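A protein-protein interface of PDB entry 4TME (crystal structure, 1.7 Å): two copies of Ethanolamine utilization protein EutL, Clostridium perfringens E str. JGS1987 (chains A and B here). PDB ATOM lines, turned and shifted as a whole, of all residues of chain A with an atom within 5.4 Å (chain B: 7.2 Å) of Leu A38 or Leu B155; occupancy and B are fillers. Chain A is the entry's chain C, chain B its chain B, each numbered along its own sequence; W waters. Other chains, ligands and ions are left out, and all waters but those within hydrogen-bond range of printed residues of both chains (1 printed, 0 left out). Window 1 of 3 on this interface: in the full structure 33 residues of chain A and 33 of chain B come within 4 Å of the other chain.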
ATOM      1  N   SER A  12      10.610 -27.213  -6.747  1.00  0.00           N
ATOM      2  CA  SER A  12       9.903 -25.953  -6.906  1.00  0.00           C
ATOM      3  C   SER A  12       8.537 -26.025  -6.257  1.00  0.00           C
ATOM      4  O   SER A  12       7.922 -27.092  -6.169  1.00  0.00           O
ATOM      5  CB  SER A  12       9.794 -25.585  -8.393  1.00  0.00           C
ATOM      6  OG  SER A  12       9.185 -24.322  -8.580  1.00  0.00           O
ATOM      7  N   VAL A  13       8.094 -24.876  -5.759  1.00  0.00           N
ATOM      8  CA  VAL A  13       6.789 -24.734  -5.131  1.00  0.00           C
ATOM      9  C   VAL A  13       6.268 -23.347  -5.421  1.00  0.00           C
ATOM     10  O   VAL A  13       6.992 -22.365  -5.248  1.00  0.00           O
ATOM     11  CB  VAL A  13       6.833 -24.923  -3.599  1.00  0.00           C
ATOM     12  CG1 VAL A  13       5.422 -24.919  -3.020  1.00  0.00           C
ATOM     13  CG2 VAL A  13       7.533 -26.191  -3.232  1.00  0.00           C
ATOM     14  N   LYS A  14       5.007 -23.250  -5.818  1.00  0.00           N
ATOM     15  CA  LYS A  14       4.400 -21.936  -6.077  1.00  0.00           C
ATOM     16  C   LYS A  14       2.900 -21.954  -5.811  1.00  0.00           C
ATOM     17  O   LYS A  14       2.266 -23.027  -5.807  1.00  0.00           O
ATOM     18  CB  LYS A  14       4.640 -21.489  -7.541  1.00  0.00           C
ATOM     19  CG  LYS A  14       6.051 -21.122  -7.898  1.00  0.00           C
ATOM     20  CD  LYS A  14       6.406 -19.749  -7.254  1.00  0.00           C
ATOM     21  CE  LYS A  14       7.859 -19.625  -7.061  1.00  0.00           C
ATOM     22  NZ  LYS A  14       8.189 -18.251  -6.595  1.00  0.00           N
ATOM     23  N   ILE A  15       2.334 -20.771  -5.579  1.00  0.00           N
ATOM     24  CA  ILE A  15       0.891 -20.633  -5.423  1.00  0.00           C
ATOM     25  C   ILE A  15       0.342 -19.745  -6.534  1.00  0.00           C
ATOM     26  O   ILE A  15       0.978 -18.762  -6.926  1.00  0.00           O
ATOM     27  CB  ILE A  15       0.514 -20.049  -4.038  1.00  0.00           C
ATOM     28  CG1 ILE A  15       0.730 -21.128  -2.978  1.00  0.00           C
ATOM     29  CG2 ILE A  15      -0.964 -19.558  -4.016  1.00  0.00           C
ATOM     30  CD1 ILE A  15       0.450 -20.675  -1.550  1.00  0.00           C
ATOM     31  N   ILE A  16      -0.809 -20.146  -7.064  1.00  0.00           N
ATOM     32  CA  ILE A  16      -1.644 -19.310  -7.927  1.00  0.00           C
ATOM     33  C   ILE A  16      -2.889 -18.909  -7.143  1.00  0.00           C
ATOM     34  O   ILE A  16      -3.699 -19.764  -6.766  1.00  0.00           O
ATOM     35  CB  ILE A  16      -2.083 -20.053  -9.229  1.00  0.00           C
ATOM     36  CG1 ILE A  16      -0.899 -20.316 -10.134  1.00  0.00           C
ATOM     37  CG2 ILE A  16      -3.180 -19.256  -9.973  1.00  0.00           C
ATOM     38  CD1 ILE A  16      -1.224 -21.275 -11.302  1.00  0.00           C
ATOM     39  N   LEU A  36      -4.561 -22.459  -6.415  1.00  0.00           N
ATOM     40  CA  LEU A  36      -3.768 -23.661  -6.695  1.00  0.00           C
ATOM     41  C   LEU A  36      -2.407 -23.618  -6.019  1.00  0.00           C
ATOM     42  O   LEU A  36      -1.787 -22.568  -5.941  1.00  0.00           O
ATOM     43  CB  LEU A  36      -3.549 -23.837  -8.203  1.00  0.00           C
ATOM     44  CG  LEU A  36      -4.795 -23.850  -9.095  1.00  0.00           C
ATOM     45  CD1 LEU A  36      -4.331 -23.969 -10.559  1.00  0.00           C
ATOM     46  CD2 LEU A  36      -5.732 -24.969  -8.722  1.00  0.00           C
ATOM     47  N   GLY A  37      -1.947 -24.770  -5.548  1.00  0.00           N
ATOM     48  CA  GLY A  37      -0.585 -24.925  -5.080  1.00  0.00           C
ATOM     49  C   GLY A  37       0.105 -25.902  -6.014  1.00  0.00           C
ATOM     50  O   GLY A  37      -0.423 -26.974  -6.285  1.00  0.00           O
ATOM     51  N   LEU A  38       1.270 -25.498  -6.520  1.00  0.00           N
ATOM     52  CA  LEU A  38       2.047 -26.231  -7.512  1.00  0.00           C
ATOM     53  C   LEU A  38       3.329 -26.769  -6.873  1.00  0.00           C
ATOM     54  O   LEU A  38       4.025 -26.018  -6.170  1.00  0.00           O
ATOM     55  CB  LEU A  38       2.422 -25.312  -8.687  1.00  0.00           C
ATOM     56  CG  LEU A  38       1.370 -24.435  -9.373  1.00  0.00           C
ATOM     57  CD1 LEU A  38       2.035 -23.468 -10.365  1.00  0.00           C
ATOM     58  CD2 LEU A  38       0.343 -25.285 -10.094  1.00  0.00           C
ATOM     59  N   ILE A  39       3.685 -28.020  -7.158  1.00  0.00           N
ATOM     60  CA  ILE A  39       4.928 -28.575  -6.649  1.00  0.00           C
ATOM     61  C   ILE A  39       5.571 -29.516  -7.655  1.00  0.00           C
ATOM     62  O   ILE A  39       4.878 -30.269  -8.347  1.00  0.00           O
ATOM     63  CB  ILE A  39       4.697 -29.311  -5.297  1.00  0.00           C
ATOM     64  CG1 ILE A  39       6.028 -29.696  -4.650  1.00  0.00           C
ATOM     65  CG2 ILE A  39       3.774 -30.502  -5.459  1.00  0.00           C
ATOM     66  CD1 ILE A  39       5.852 -30.146  -3.180  1.00  0.00           C
ATOM     67  N   THR A  40       6.899 -29.447  -7.745  1.00  0.00           N
ATOM     68  CA  THR A  40       7.682 -30.458  -8.458  1.00  0.00           C
ATOM     69  C   THR A  40       8.778 -30.992  -7.563  1.00  0.00           C
ATOM     70  O   THR A  40       9.231 -30.322  -6.627  1.00  0.00           O
ATOM     71  CB  THR A  40       8.328 -29.930  -9.761  1.00  0.00           C
ATOM     72  OG1 THR A  40       9.329 -28.961  -9.455  1.00  0.00           O
ATOM     73  CG2 THR A  40       7.287 -29.306 -10.672  1.00  0.00           C
ATOM     74  N   ILE A  84       4.865 -33.454 -11.313  1.00  0.00           N
ATOM     75  CA  ILE A  84       4.174 -32.199 -11.016  1.00  0.00           C
ATOM     76  C   ILE A  84       2.886 -32.547 -10.280  1.00  0.00           C
ATOM     77  O   ILE A  84       2.126 -33.455 -10.670  1.00  0.00           O
ATOM     78  CB  ILE A  84       3.874 -31.344 -12.277  1.00  0.00           C
ATOM     79  CG1 ILE A  84       3.195 -30.027 -11.811  1.00  0.00           C
ATOM     80  CG2 ILE A  84       3.064 -32.153 -13.315  1.00  0.00           C
ATOM     81  CD1 ILE A  84       3.196 -28.935 -12.793  1.00  0.00           C
ATOM     82  N   GLY A  85       2.665 -31.861  -9.159  1.00  0.00           N
ATOM     83  CA  GLY A  85       1.460 -32.031  -8.381  1.00  0.00           C
ATOM     84  C   GLY A  85       0.744 -30.695  -8.249  1.00  0.00           C
ATOM     85  O   GLY A  85       1.403 -29.654  -8.133  1.00  0.00           O
ATOM     86  N   ILE A  86      -0.587 -30.710  -8.311  1.00  0.00           N
ATOM     87  CA  ILE A  86      -1.374 -29.500  -8.103  1.00  0.00           C
ATOM     88  C   ILE A  86      -2.454 -29.739  -7.071  1.00  0.00           C
ATOM     89  O   ILE A  86      -3.299 -30.637  -7.209  1.00  0.00           O
ATOM     90  CB  ILE A  86      -2.032 -28.988  -9.417  1.00  0.00           C
ATOM     91  CG1 ILE A  86      -0.958 -28.737 -10.471  1.00  0.00           C
ATOM     92  CG2 ILE A  86      -2.815 -27.661  -9.153  1.00  0.00           C
ATOM     93  CD1 ILE A  86      -1.467 -28.238 -11.824  1.00  0.00           C
ATOM     94  N   LEU A  87      -2.391 -28.940  -6.011  1.00  0.00           N
ATOM     95  CA  LEU A  87      -3.422 -28.877  -4.987  1.00  0.00           C
ATOM     96  C   LEU A  87      -4.380 -27.745  -5.309  1.00  0.00           C
ATOM     97  O   LEU A  87      -3.957 -26.714  -5.823  1.00  0.00           O
ATOM     98  CB  LEU A  87      -2.808 -28.622  -3.603  1.00  0.00           C
ATOM     99  CG  LEU A  87      -1.905 -29.715  -3.042  1.00  0.00           C
ATOM    100  CD1 LEU A  87      -1.244 -29.166  -1.771  1.00  0.00           C
ATOM    101  CD2 LEU A  87      -2.717 -30.943  -2.713  1.00  0.00           C
ATOM    102  N   LEU A  99       0.519 -27.118   1.031  1.00  0.00           N
ATOM    103  CA  LEU A  99       1.867 -27.239   0.493  1.00  0.00           C
ATOM    104  C   LEU A  99       2.876 -27.431   1.632  1.00  0.00           C
ATOM    105  O   LEU A  99       3.807 -28.215   1.505  1.00  0.00           O
ATOM    106  CB  LEU A  99       2.234 -26.013  -0.339  1.00  0.00           C
ATOM    107  CG  LEU A  99       1.564 -25.883  -1.710  1.00  0.00           C
ATOM    108  CD1 LEU A  99       1.822 -24.488  -2.297  1.00  0.00           C
ATOM    109  CD2 LEU A  99       2.063 -26.968  -2.677  1.00  0.00           C
ATOM    110  N   ALA B 152       7.034 -23.841 -21.474  1.00  0.00           N
ATOM    111  CA  ALA B 152       8.062 -23.839 -20.416  1.00  0.00           C
ATOM    112  C   ALA B 152       8.032 -25.180 -19.687  1.00  0.00           C
ATOM    113  O   ALA B 152       7.129 -25.999 -19.917  1.00  0.00           O
ATOM    114  CB  ALA B 152       7.840 -22.667 -19.438  1.00  0.00           C
ATOM    115  N   PRO B 153       9.003 -25.430 -18.783  1.00  0.00           N
ATOM    116  CA  PRO B 153       8.853 -26.690 -18.041  1.00  0.00           C
ATOM    117  C   PRO B 153       7.582 -26.678 -17.181  1.00  0.00           C
ATOM    118  O   PRO B 153       6.965 -25.623 -17.034  1.00  0.00           O
ATOM    119  CB  PRO B 153      10.147 -26.760 -17.206  1.00  0.00           C
ATOM    120  CG  PRO B 153      11.108 -25.873 -17.932  1.00  0.00           C
ATOM    121  CD  PRO B 153      10.250 -24.740 -18.446  1.00  0.00           C
ATOM    122  N   PRO B 154       7.169 -27.837 -16.647  1.00  0.00           N
ATOM    123  CA  PRO B 154       5.814 -27.992 -16.104  1.00  0.00           C
ATOM    124  C   PRO B 154       5.336 -26.946 -15.098  1.00  0.00           C
ATOM    125  O   PRO B 154       4.309 -26.320 -15.364  1.00  0.00           O
ATOM    126  CB  PRO B 154       5.875 -29.386 -15.464  1.00  0.00           C
ATOM    127  CG  PRO B 154       6.790 -30.127 -16.450  1.00  0.00           C
ATOM    128  CD  PRO B 154       7.895 -29.122 -16.675  1.00  0.00           C
ATOM    129  N   LEU B 155       6.042 -26.724 -13.996  1.00  0.00           N
ATOM    130  CA  LEU B 155       5.525 -25.811 -12.994  1.00  0.00           C
ATOM    131  C   LEU B 155       5.605 -24.393 -13.497  1.00  0.00           C
ATOM    132  O   LEU B 155       4.635 -23.626 -13.360  1.00  0.00           O
ATOM    133  CB  LEU B 155       6.287 -25.961 -11.672  1.00  0.00           C
ATOM    134  CG  LEU B 155       5.759 -25.099 -10.528  1.00  0.00           C
ATOM    135  CD1 LEU B 155       5.880 -25.831  -9.201  1.00  0.00           C
ATOM    136  CD2 LEU B 155       6.559 -23.805 -10.483  1.00  0.00           C
ATOM    137  N   GLU B 156       6.747 -24.045 -14.088  1.00  0.00           N
ATOM    138  CA  GLU B 156       6.928 -22.698 -14.648  1.00  0.00           C
ATOM    139  C   GLU B 156       5.790 -22.392 -15.624  1.00  0.00           C
ATOM    140  O   GLU B 156       5.264 -21.290 -15.653  1.00  0.00           O
ATOM    141  CB  GLU B 156       8.270 -22.566 -15.368  1.00  0.00           C
ATOM    142  CG  GLU B 156       9.475 -22.741 -14.481  1.00  0.00           C
ATOM    143  CD  GLU B 156      10.019 -24.163 -14.523  1.00  0.00           C
ATOM    144  OE1 GLU B 156       9.220 -25.108 -14.307  1.00  0.00           O
ATOM    145  OE2 GLU B 156      11.219 -24.321 -14.815  1.00  0.00           O
ATOM    146  N   ALA B 157       5.463 -23.362 -16.472  1.00  0.00           N
ATOM    147  CA  ALA B 157       4.438 -23.137 -17.473  1.00  0.00           C
ATOM    148  C   ALA B 157       3.073 -22.871 -16.843  1.00  0.00           C
ATOM    149  O   ALA B 157       2.343 -21.997 -17.304  1.00  0.00           O
ATOM    150  CB  ALA B 157       4.362 -24.326 -18.435  1.00  0.00           C
ATOM    151  N   MET B 158       2.715 -23.624 -15.813  1.00  0.00           N
ATOM    152  CA  MET B 158       1.405 -23.449 -15.192  1.00  0.00           C
ATOM    153  C   MET B 158       1.334 -22.063 -14.523  1.00  0.00           C
ATOM    154  O   MET B 158       0.356 -21.302 -14.685  1.00  0.00           O
ATOM    155  CB  MET B 158       1.137 -24.550 -14.166  1.00  0.00           C
ATOM    156  CG  MET B 158       1.075 -25.974 -14.713  1.00  0.00           C
ATOM    157  SD  MET B 158      -0.151 -26.142 -16.036  1.00  0.00           S
ATOM    158  CE  MET B 158      -1.655 -25.761 -15.154  1.00  0.00           C
ATOM    159  N   TYR B 159       2.374 -21.734 -13.760  1.00  0.00           N
ATOM    160  CA  TYR B 159       2.465 -20.436 -13.075  1.00  0.00           C
ATOM    161  C   TYR B 159       2.440 -19.266 -14.080  1.00  0.00           C
ATOM    162  O   TYR B 159       1.728 -18.269 -13.890  1.00  0.00           O
ATOM    163  CB  TYR B 159       3.753 -20.405 -12.267  1.00  0.00           C
ATOM    164  CG  TYR B 159       3.972 -19.193 -11.413  1.00  0.00           C
ATOM    165  CD1 TYR B 159       3.396 -19.116 -10.164  1.00  0.00           C
ATOM    166  CD2 TYR B 159       4.762 -18.135 -11.853  1.00  0.00           C
ATOM    167  CE1 TYR B 159       3.609 -18.005  -9.357  1.00  0.00           C
ATOM    168  CE2 TYR B 159       4.980 -17.021 -11.047  1.00  0.00           C
ATOM    169  CZ  TYR B 159       4.400 -16.972  -9.818  1.00  0.00           C
ATOM    170  OH  TYR B 159       4.621 -15.882  -9.013  1.00  0.00           O
ATOM    171  N   ALA B 160       3.213 -19.412 -15.157  1.00  0.00           N
ATOM    172  CA  ALA B 160       3.380 -18.329 -16.125  1.00  0.00           C
ATOM    173  C   ALA B 160       2.158 -18.201 -17.052  1.00  0.00           C
ATOM    174  O   ALA B 160       1.858 -17.119 -17.528  1.00  0.00           O
ATOM    175  CB  ALA B 160       4.645 -18.524 -16.931  1.00  0.00           C
ATOM    176  N   LEU B 161       1.454 -19.298 -17.315  1.00  0.00           N
ATOM    177  CA  LEU B 161       0.207 -19.203 -18.073  1.00  0.00           C
ATOM    178  C   LEU B 161      -0.826 -18.392 -17.320  1.00  0.00           C
ATOM    179  O   LEU B 161      -1.523 -17.565 -17.900  1.00  0.00           O
ATOM    180  CB  LEU B 161      -0.366 -20.590 -18.401  1.00  0.00           C
ATOM    181  CG  LEU B 161       0.291 -21.360 -19.546  1.00  0.00           C
ATOM    182  CD1 LEU B 161      -0.342 -22.738 -19.630  1.00  0.00           C
ATOM    183  CD2 LEU B 161       0.198 -20.639 -20.902  1.00  0.00           C
ATOM    184  N   PRO B 178       1.084 -30.884 -18.766  1.00  0.00           N
ATOM    185  CA  PRO B 178       2.375 -31.485 -18.402  1.00  0.00           C
ATOM    186  C   PRO B 178       2.236 -32.935 -17.961  1.00  0.00           C
ATOM    187  O   PRO B 178       1.377 -33.263 -17.138  1.00  0.00           O
ATOM    188  CB  PRO B 178       2.855 -30.624 -17.230  1.00  0.00           C
ATOM    189  CG  PRO B 178       1.641 -30.048 -16.657  1.00  0.00           C
ATOM    190  CD  PRO B 178       0.649 -29.873 -17.797  1.00  0.00           C
ATOM    191  N   ALA B 185       5.372 -28.039 -21.073  1.00  0.00           N
ATOM    192  CA  ALA B 185       3.944 -27.730 -20.987  1.00  0.00           C
ATOM    193  C   ALA B 185       3.729 -26.309 -21.466  1.00  0.00           C
ATOM    194  O   ALA B 185       4.687 -25.602 -21.768  1.00  0.00           O
ATOM    195  CB  ALA B 185       3.428 -27.894 -19.554  1.00  0.00           C
ATOM    196  N   VAL B 210      10.048 -17.452 -11.506  1.00  0.00           N
ATOM    197  CA  VAL B 210      10.140 -18.773 -10.865  1.00  0.00           C
ATOM    198  C   VAL B 210      11.616 -19.223 -10.820  1.00  0.00           C
ATOM    199  O   VAL B 210      12.098 -19.723  -9.804  1.00  0.00           O
ATOM    200  CB  VAL B 210       9.272 -19.839 -11.596  1.00  0.00           C
ATOM    201  CG1 VAL B 210       9.430 -21.196 -10.929  1.00  0.00           C
ATOM    202  CG2 VAL B 210       7.805 -19.412 -11.547  1.00  0.00           C
ATOM    203  N   PRO B 214      12.636 -20.364  -6.875  1.00  0.00           N
ATOM    204  CA  PRO B 214      11.819 -21.547  -7.231  1.00  0.00           C
ATOM    205  C   PRO B 214      11.026 -22.130  -6.083  1.00  0.00           C
ATOM    206  O   PRO B 214      10.013 -22.790  -6.368  1.00  0.00           O
ATOM    207  CB  PRO B 214      12.853 -22.557  -7.749  1.00  0.00           C
ATOM    208  CG  PRO B 214      14.176 -22.042  -7.302  1.00  0.00           C
ATOM    209  CD  PRO B 214      14.066 -20.554  -7.153  1.00  0.00           C
ATOM    210  N   PHE B 217       6.872 -19.399  -1.715  1.00  0.00           N
ATOM    211  CA  PHE B 217       5.408 -19.337  -1.851  1.00  0.00           C
ATOM    212  C   PHE B 217       4.686 -18.722  -0.668  1.00  0.00           C
ATOM    213  O   PHE B 217       3.461 -18.711  -0.650  1.00  0.00           O
ATOM    214  CB  PHE B 217       4.841 -20.761  -2.112  1.00  0.00           C
ATOM    215  CG  PHE B 217       4.952 -21.697  -0.936  1.00  0.00           C
ATOM    216  CD1 PHE B 217       6.164 -22.284  -0.613  1.00  0.00           C
ATOM    217  CD2 PHE B 217       3.852 -21.980  -0.130  1.00  0.00           C
ATOM    218  CE1 PHE B 217       6.266 -23.144   0.461  1.00  0.00           C
ATOM    219  CE2 PHE B 217       3.951 -22.833   0.941  1.00  0.00           C
ATOM    220  CZ  PHE B 217       5.157 -23.418   1.254  1.00  0.00           C
HETATM  221  O   HOH W   1       7.638 -16.291  -8.587  1.00  0.00           O
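The side-chain hydroxyl (OG) of Ser A12 lies within hydrogen-bond range of the backbone carbonyl oxygen (O) of Pro B214, at 2.8 Å. The backbone NH (N) of Val A13 lies within hydrogen-bond range of the backbone carbonyl oxygen (O) of Pro B214.
The backbone NH (N) of Thr A40 is in hydrogen-bond range of the backbone carbonyl oxygen (O) of Ser A12, at 3.0 Å. The backbone carbonyl oxygen of Lys A14 sits at hydrogen-bond distance from the backbone NH of Leu A38 (2.8 Å). The backbone carbonyl oxygen (O) of Leu A36 sits at hydrogen-bond distance from the backbone NH (N) of Ile A16 (2.8 Å). N of Gly A85 sits at hydrogen-bond distance from O of Ile A39 (2.8 Å).
OG of Ser A12 touches CD2 of Leu B155, 3.3 Å away. CD1 of Phe B217 touches CG1 of Val A13 (3.6 Å). CB of Lys A14 touches CD1 of Tyr B159, 3.7 Å away. Tyr B159 touches Ile A15. Phe B217 touches Ile A15 (O to CD1, 3.7 Å). O of Met B158 touches CD1 of Ile A16 (3.7 Å). CD1 of Leu B155 touches CB of Leu A38, 3.5 Å away. Thr A40 touches Leu B155. C of Pro B154 touches CD1 of Ile A84, at 3.7 Å. Phe B217 touches Leu A99.
Of the printed residues of chain B, Leu A38 touches Leu B155 (3.5 Å) and Tyr B159 (3.8 Å). Of the printed residues of chain A, Leu B155 touches Ser A12 (3.3 Å), Lys A14 (3.8 Å), Leu A38 (3.5 Å), Ile A39 (3.7 Å), Thr A40 (3.6 Å) and Ile A84 (3.8 Å). Printed residues of chain B within 4 Å of Leu A99: Phe B217 (3.8 Å). Printed residues of chain B within 4 Å of Ser A12: Leu B155 (3.3 Å), Val B210 (3.9 Å) and Pro B214 (2.8 Å). Of the printed residues of chain A, Pro B214 touches Ser A12, Val A13 and Lys A14. Printed residues of chain A within 4 Å of Phe B217: Val A13 (3.6 Å), Ile A15 (3.7 Å) and Leu A99 (3.8 Å). Printed residues of chain B within 4 Å of Val A13: Pro B214 (2.9 Å) and Phe B217 (3.6 Å). The nearest printed residue of chain B that does not touch Leu A38 is Met B158 (4.1 Å). The nearest printed residue of chain B that does not touch Ile A84 is Met B158 (4.1 Å).
Printed residues of chain A that touch a printed residue of chain B: Ser A12, Val A13, Lys A14, Ile A15, Ile A16, Leu A38, Ile A39, Thr A40, Ile A84 and Leu A99. Hydrophobic or aromatic side chains of chain A within 4 Å of the printed part of chain B: Val A13, Ile A15, Ile A16, Leu A38, Ile A84 and Leu A99. Of the 15 printed residues of chain B, 7 touch a printed residue of chain A. Printed residues of chain B that touch a printed residue of chain A: Pro B154, Leu B155, Met B158, Tyr B159, Val B210, Pro B214 and Phe B217. Among the printed residues, 18 pairs touch across the chains.
No position is printed for both chains. Of the 18 pairs that touch across the chains among the printed residues, none has its exchanged pair printed and touching as well.
Water W1 lies within hydrogen-bond range of NZ of Lys A14 (2.8 Å) and OH of Tyr B159 (3.1 Å).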
